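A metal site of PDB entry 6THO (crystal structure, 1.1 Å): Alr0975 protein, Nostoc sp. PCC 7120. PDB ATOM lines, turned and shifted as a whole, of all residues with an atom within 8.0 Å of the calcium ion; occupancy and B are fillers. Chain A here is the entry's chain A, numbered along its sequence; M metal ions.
ND2 of Asn 139 is in hydrogen-bond range of O of Phe 146.
Within 4 Å of the calcium ion: Asp 33, Asn 139, Gln 142 and Asn 145.
The calcium ion is bound by O of Asn 139 (2.3 Å), O of Asn 145 (2.3 Å), O of Gln 142 (2.3 Å), OD1 of Asn 145 (2.3 Å), OD1 of Asp 33 (2.4 Å), OD1 of Asn 139 (2.5 Å) and OD2 of Asp 33 (2.5 Å).
The calcium ion has seven donor atoms within binding distance.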
ATOM      1  N   ARG A  31      27.073   7.904  18.982  1.00  0.00           N
ATOM      2  CA  ARG A  31      28.473   8.110  18.614  1.00  0.00           C
ATOM      3  C   ARG A  31      28.883   7.291  17.406  1.00  0.00           C
ATOM      4  O   ARG A  31      30.085   7.118  17.166  1.00  0.00           O
ATOM      5  CB  ARG A  31      29.362   7.738  19.807  1.00  0.00           C
ATOM      6  CG  ARG A  31      29.193   6.281  20.235  1.00  0.00           C
ATOM      7  CD  ARG A  31      30.120   5.876  21.372  1.00  0.00           C
ATOM      8  NE  ARG A  31      29.808   4.494  21.759  1.00  0.00           N
ATOM      9  CZ  ARG A  31      30.084   3.965  22.949  1.00  0.00           C
ATOM     10  NH1 ARG A  31      29.719   2.710  23.191  1.00  0.00           N
ATOM     11  NH2 ARG A  31      30.720   4.660  23.868  1.00  0.00           N
ATOM     12  N   GLU A  32      27.931   6.772  16.627  1.00  0.00           N
ATOM     13  CA  GLU A  32      28.294   5.968  15.462  1.00  0.00           C
ATOM     14  C   GLU A  32      29.162   6.754  14.493  1.00  0.00           C
ATOM     15  O   GLU A  32      30.094   6.213  13.894  1.00  0.00           O
ATOM     16  CB  GLU A  32      27.033   5.459  14.765  1.00  0.00           C
ATOM     17  CG  GLU A  32      26.271   4.437  15.558  1.00  0.00           C
ATOM     18  CD  GLU A  32      27.163   3.356  16.103  1.00  0.00           C
ATOM     19  OE1 GLU A  32      27.342   3.306  17.346  1.00  0.00           O
ATOM     20  OE2 GLU A  32      27.713   2.578  15.300  1.00  0.00           O
ATOM     21  N   ASP A  33      28.870   8.043  14.329  1.00  0.00           N
ATOM     22  CA  ASP A  33      29.585   8.837  13.333  1.00  0.00           C
ATOM     23  C   ASP A  33      31.023   9.129  13.748  1.00  0.00           C
ATOM     24  O   ASP A  33      31.851   9.461  12.885  1.00  0.00           O
ATOM     25  CB  ASP A  33      28.863  10.156  13.077  1.00  0.00           C
ATOM     26  CG  ASP A  33      27.504   9.992  12.413  1.00  0.00           C
ATOM     27  OD1 ASP A  33      27.134   8.845  12.035  1.00  0.00           O
ATOM     28  OD2 ASP A  33      26.792  11.020  12.283  1.00  0.00           O
ATOM     29  N   PHE A  34      31.335   9.013  15.036  1.00  0.00           N
ATOM     30  CA  PHE A  34      32.682   9.335  15.499  1.00  0.00           C
ATOM     31  C   PHE A  34      33.719   8.481  14.788  1.00  0.00           C
ATOM     32  O   PHE A  34      34.787   8.967  14.392  1.00  0.00           O
ATOM     33  CB  PHE A  34      32.824   9.159  17.025  1.00  0.00           C
ATOM     34  CG  PHE A  34      34.260   9.231  17.452  1.00  0.00           C
ATOM     35  CD1 PHE A  34      34.913  10.444  17.533  1.00  0.00           C
ATOM     36  CD2 PHE A  34      34.994   8.083  17.673  1.00  0.00           C
ATOM     37  CE1 PHE A  34      36.268  10.507  17.830  1.00  0.00           C
ATOM     38  CE2 PHE A  34      36.338   8.135  17.965  1.00  0.00           C
ATOM     39  CZ  PHE A  34      36.977   9.342  18.047  1.00  0.00           C
ATOM     40  N   PRO A  36      33.935   6.685  11.737  1.00  0.00           N
ATOM     41  CA  PRO A  36      34.349   7.073  10.380  1.00  0.00           C
ATOM     42  C   PRO A  36      34.916   8.485  10.302  1.00  0.00           C
ATOM     43  O   PRO A  36      35.870   8.712   9.555  1.00  0.00           O
ATOM     44  CB  PRO A  36      33.061   6.910   9.547  1.00  0.00           C
ATOM     45  CG  PRO A  36      31.959   6.926  10.521  1.00  0.00           C
ATOM     46  CD  PRO A  36      32.516   6.295  11.779  1.00  0.00           C
ATOM     47  N   LEU A  37      34.355   9.441  11.045  1.00  0.00           N
ATOM     48  CA  LEU A  37      34.890  10.801  10.963  1.00  0.00           C
ATOM     49  C   LEU A  37      36.322  10.837  11.486  1.00  0.00           C
ATOM     50  O   LEU A  37      37.170  11.547  10.920  1.00  0.00           O
ATOM     51  CB  LEU A  37      34.026  11.807  11.718  1.00  0.00           C
ATOM     52  CG  LEU A  37      32.657  12.107  11.074  1.00  0.00           C
ATOM     53  CD1 LEU A  37      31.793  12.875  12.040  1.00  0.00           C
ATOM     54  CD2 LEU A  37      32.812  12.843   9.766  1.00  0.00           C
ATOM     55  N   LEU A  62      31.380   8.790   3.746  1.00  0.00           N
ATOM     56  CA  LEU A  62      30.256   8.204   3.025  1.00  0.00           C
ATOM     57  C   LEU A  62      30.697   7.311   1.886  1.00  0.00           C
ATOM     58  O   LEU A  62      29.858   6.659   1.268  1.00  0.00           O
ATOM     59  CB  LEU A  62      29.341   9.309   2.495  1.00  0.00           C
ATOM     60  CG  LEU A  62      28.478  10.022   3.534  1.00  0.00           C
ATOM     61  CD1 LEU A  62      27.875  11.282   2.930  1.00  0.00           C
ATOM     62  CD2 LEU A  62      27.388   9.100   4.053  1.00  0.00           C
ATOM     63  N   GLN A 135      16.969  15.712  16.371  1.00  0.00           N
ATOM     64  CA  GLN A 135      17.276  15.221  15.038  1.00  0.00           C
ATOM     65  C   GLN A 135      18.759  14.929  14.880  1.00  0.00           C
ATOM     66  O   GLN A 135      19.156  13.961  14.203  1.00  0.00           O
ATOM     67  CB  GLN A 135      16.825  16.237  13.984  1.00  0.00           C
ATOM     68  CG  GLN A 135      15.305  16.424  13.931  1.00  0.00           C
ATOM     69  CD  GLN A 135      14.887  17.621  13.115  1.00  0.00           C
ATOM     70  OE1 GLN A 135      15.708  18.281  12.479  1.00  0.00           O
ATOM     71  NE2 GLN A 135      13.605  17.928  13.146  1.00  0.00           N
ATOM     72  N   VAL A 136      19.611  15.737  15.502  1.00  0.00           N
ATOM     73  CA  VAL A 136      21.053  15.509  15.401  1.00  0.00           C
ATOM     74  C   VAL A 136      21.456  14.292  16.215  1.00  0.00           C
ATOM     75  O   VAL A 136      22.239  13.457  15.751  1.00  0.00           O
ATOM     76  CB  VAL A 136      21.833  16.777  15.767  1.00  0.00           C
ATOM     77  CG1 VAL A 136      23.330  16.493  15.818  1.00  0.00           C
ATOM     78  CG2 VAL A 136      21.544  17.877  14.745  1.00  0.00           C
ATOM     79  N   ALA A 137      20.924  14.150  17.434  1.00  0.00           N
ATOM     80  CA  ALA A 137      21.232  12.954  18.224  1.00  0.00           C
ATOM     81  C   ALA A 137      20.821  11.684  17.477  1.00  0.00           C
ATOM     82  O   ALA A 137      21.534  10.668  17.531  1.00  0.00           O
ATOM     83  CB  ALA A 137      20.541  13.035  19.578  1.00  0.00           C
ATOM     84  N   GLU A 138      19.691  11.720  16.776  1.00  0.00           N
ATOM     85  CA  GLU A 138      19.269  10.561  15.987  1.00  0.00           C
ATOM     86  C   GLU A 138      20.260  10.283  14.864  1.00  0.00           C
ATOM     87  O   GLU A 138      20.693   9.145  14.668  1.00  0.00           O
ATOM     88  CB  GLU A 138      17.845  10.786  15.460  1.00  0.00           C
ATOM     89  CG  GLU A 138      17.376   9.711  14.512  1.00  0.00           C
ATOM     90  CD  GLU A 138      15.968   9.975  13.995  1.00  0.00           C
ATOM     91  OE1 GLU A 138      15.621  11.153  13.767  1.00  0.00           O
ATOM     92  OE2 GLU A 138      15.214   9.000  13.813  1.00  0.00           O
ATOM     93  N   ASN A 139      20.653  11.318  14.111  1.00  0.00           N
ATOM     94  CA  ASN A 139      21.634  11.125  13.061  1.00  0.00           C
ATOM     95  C   ASN A 139      22.922  10.525  13.619  1.00  0.00           C
ATOM     96  O   ASN A 139      23.516   9.622  13.012  1.00  0.00           O
ATOM     97  CB  ASN A 139      21.885  12.461  12.342  1.00  0.00           C
ATOM     98  CG  ASN A 139      22.901  12.363  11.206  1.00  0.00           C
ATOM     99  OD1 ASN A 139      24.005  11.913  11.388  1.00  0.00           O
ATOM    100  ND2 ASN A 139      22.530  12.847  10.032  1.00  0.00           N
ATOM    101  N   LEU A 140      23.363  10.981  14.789  1.00  0.00           N
ATOM    102  CA  LEU A 140      24.630  10.504  15.334  1.00  0.00           C
ATOM    103  C   LEU A 140      24.589   9.020  15.706  1.00  0.00           C
ATOM    104  O   LEU A 140      25.652   8.408  15.816  1.00  0.00           O
ATOM    105  CB  LEU A 140      25.094  11.408  16.490  1.00  0.00           C
ATOM    106  CG  LEU A 140      25.462  12.820  16.038  1.00  0.00           C
ATOM    107  CD1 LEU A 140      25.639  13.728  17.248  1.00  0.00           C
ATOM    108  CD2 LEU A 140      26.708  12.826  15.183  1.00  0.00           C
ATOM    109  N   LYS A 141      23.388   8.430  15.857  1.00  0.00           N
ATOM    110  CA  LYS A 141      23.233   6.991  16.075  1.00  0.00           C
ATOM    111  C   LYS A 141      23.188   6.205  14.779  1.00  0.00           C
ATOM    112  O   LYS A 141      23.187   4.957  14.817  1.00  0.00           O
ATOM    113  CB  LYS A 141      21.924   6.688  16.807  1.00  0.00           C
ATOM    114  CG  LYS A 141      21.861   7.190  18.225  1.00  0.00           C
ATOM    115  CD  LYS A 141      20.550   6.751  18.859  1.00  0.00           C
ATOM    116  CE  LYS A 141      20.425   7.287  20.260  1.00  0.00           C
ATOM    117  NZ  LYS A 141      20.281   8.757  20.216  1.00  0.00           N
ATOM    118  N   GLN A 142      23.113   6.880  13.643  1.00  0.00           N
ATOM    119  CA  GLN A 142      22.833   6.241  12.357  1.00  0.00           C
ATOM    120  C   GLN A 142      24.063   6.293  11.460  1.00  0.00           C
ATOM    121  O   GLN A 142      24.679   7.354  11.303  1.00  0.00           O
ATOM    122  CB  GLN A 142      21.668   6.940  11.637  1.00  0.00           C
ATOM    123  CG  GLN A 142      20.332   6.833  12.359  1.00  0.00           C
ATOM    124  CD  GLN A 142      19.276   7.760  11.775  1.00  0.00           C
ATOM    125  OE1 GLN A 142      19.578   8.739  11.102  1.00  0.00           O
ATOM    126  NE2 GLN A 142      18.019   7.461  12.066  1.00  0.00           N
ATOM    127  N   ASP A 143      24.393   5.155  10.872  1.00  0.00           N
ATOM    128  CA  ASP A 143      25.388   5.118   9.825  1.00  0.00           C
ATOM    129  C   ASP A 143      24.797   5.668   8.522  1.00  0.00           C
ATOM    130  O   ASP A 143      23.581   5.777   8.362  1.00  0.00           O
ATOM    131  CB  ASP A 143      25.853   3.682   9.594  1.00  0.00           C
ATOM    132  CG  ASP A 143      26.653   3.126  10.764  1.00  0.00           C
ATOM    133  OD1 ASP A 143      27.350   3.889  11.468  1.00  0.00           O
ATOM    134  OD2 ASP A 143      26.574   1.893  10.971  1.00  0.00           O
ATOM    135  N   GLY A 144      25.682   6.051   7.603  1.00  0.00           N
ATOM    136  CA  GLY A 144      25.259   6.487   6.286  1.00  0.00           C
ATOM    137  C   GLY A 144      24.793   7.924   6.199  1.00  0.00           C
ATOM    138  O   GLY A 144      24.272   8.346   5.163  1.00  0.00           O
ATOM    139  N   ASN A 145      24.944   8.700   7.261  1.00  0.00           N
ATOM    140  CA  ASN A 145      24.565  10.100   7.263  1.00  0.00           C
ATOM    141  C   ASN A 145      25.421  10.819   8.304  1.00  0.00           C
ATOM    142  O   ASN A 145      25.967  10.187   9.217  1.00  0.00           O
ATOM    143  CB  ASN A 145      23.057  10.317   7.465  1.00  0.00           C
ATOM    144  CG  ASN A 145      22.518   9.707   8.756  1.00  0.00           C
ATOM    145  OD1 ASN A 145      23.213   9.560   9.745  1.00  0.00           O
ATOM    146  ND2 ASN A 145      21.248   9.387   8.745  1.00  0.00           N
ATOM    147  N   PHE A 146      25.553  12.139   8.128  1.00  0.00           N
ATOM    148  CA  PHE A 146      26.440  12.944   8.958  1.00  0.00           C
ATOM    149  C   PHE A 146      25.828  14.316   9.157  1.00  0.00           C
ATOM    150  O   PHE A 146      24.872  14.704   8.478  1.00  0.00           O
ATOM    151  CB  PHE A 146      27.848  13.033   8.320  1.00  0.00           C
ATOM    152  CG  PHE A 146      28.544  11.713   8.294  1.00  0.00           C
ATOM    153  CD1 PHE A 146      29.213  11.253   9.407  1.00  0.00           C
ATOM    154  CD2 PHE A 146      28.428  10.879   7.195  1.00  0.00           C
ATOM    155  CE1 PHE A 146      29.789  10.003   9.442  1.00  0.00           C
ATOM    156  CE2 PHE A 146      28.985   9.601   7.235  1.00  0.00           C
ATOM    157  CZ  PHE A 146      29.665   9.173   8.364  1.00  0.00           C
ATOM    158  N   VAL A 147      26.423  15.059  10.094  1.00  0.00           N
ATOM    159  CA  VAL A 147      25.987  16.399  10.437  1.00  0.00           C
ATOM    160  C   VAL A 147      27.195  17.341  10.444  1.00  0.00           C
ATOM    161  O   VAL A 147      28.220  17.025  11.051  1.00  0.00           O
ATOM    162  CB  VAL A 147      25.326  16.440  11.832  1.00  0.00           C
ATOM    163  CG1 VAL A 147      24.774  17.839  12.114  1.00  0.00           C
ATOM    164  CG2 VAL A 147      24.293  15.342  11.981  1.00  0.00           C
ATOM    165  N   LEU A 167      30.000  17.332  13.445  1.00  0.00           N
ATOM    166  CA  LEU A 167      29.694  16.759  14.756  1.00  0.00           C
ATOM    167  C   LEU A 167      29.913  15.252  14.729  1.00  0.00           C
ATOM    168  O   LEU A 167      29.576  14.581  13.749  1.00  0.00           O
ATOM    169  CB  LEU A 167      28.250  17.000  15.190  1.00  0.00           C
ATOM    170  CG  LEU A 167      27.869  18.454  15.358  1.00  0.00           C
ATOM    171  CD1 LEU A 167      26.428  18.549  15.835  1.00  0.00           C
ATOM    172  CD2 LEU A 167      28.770  19.207  16.314  1.00  0.00           C
ATOM    173  N   ALA A 168      30.438  14.704  15.818  1.00  0.00           N
ATOM    174  CA  ALA A 168      30.788  13.278  15.871  1.00  0.00           C
ATOM    175  C   ALA A 168      30.001  12.483  16.905  1.00  0.00           C
ATOM    176  O   ALA A 168      29.930  11.256  16.752  1.00  0.00           O
ATOM    177  CB  ALA A 168      32.282  13.110  16.155  1.00  0.00           C
ATOM    178  N   PHE A 216      22.490  18.274   7.310  1.00  0.00           N
ATOM    179  CA  PHE A 216      22.480  16.821   7.280  1.00  0.00           C
ATOM    180  C   PHE A 216      22.918  16.367   5.892  1.00  0.00           C
ATOM    181  O   PHE A 216      22.475  16.925   4.879  1.00  0.00           O
ATOM    182  CB  PHE A 216      21.080  16.286   7.566  1.00  0.00           C
ATOM    183  CG  PHE A 216      20.596  16.551   8.956  1.00  0.00           C
ATOM    184  CD1 PHE A 216      21.338  16.133  10.051  1.00  0.00           C
ATOM    185  CD2 PHE A 216      19.408  17.212   9.175  1.00  0.00           C
ATOM    186  CE1 PHE A 216      20.893  16.359  11.324  1.00  0.00           C
ATOM    187  CE2 PHE A 216      18.971  17.442  10.459  1.00  0.00           C
ATOM    188  CZ  PHE A 216      19.716  17.011  11.538  1.00  0.00           C
ATOM    189  N   VAL A 217      23.777  15.358   5.840  1.00  0.00           N
ATOM    190  CA  VAL A 217      24.338  14.838   4.600  1.00  0.00           C
ATOM    191  C   VAL A 217      24.166  13.331   4.580  1.00  0.00           C
ATOM    192  O   VAL A 217      24.461  12.658   5.565  1.00  0.00           O
ATOM    193  CB  VAL A 217      25.844  15.165   4.499  1.00  0.00           C
ATOM    194  CG1 VAL A 217      26.357  14.830   3.107  1.00  0.00           C
ATOM    195  CG2 VAL A 217      26.137  16.622   4.838  1.00  0.00           C
HETATM  196 CA    CA M   1      24.992   9.661  11.253  1.00  0.00          CA
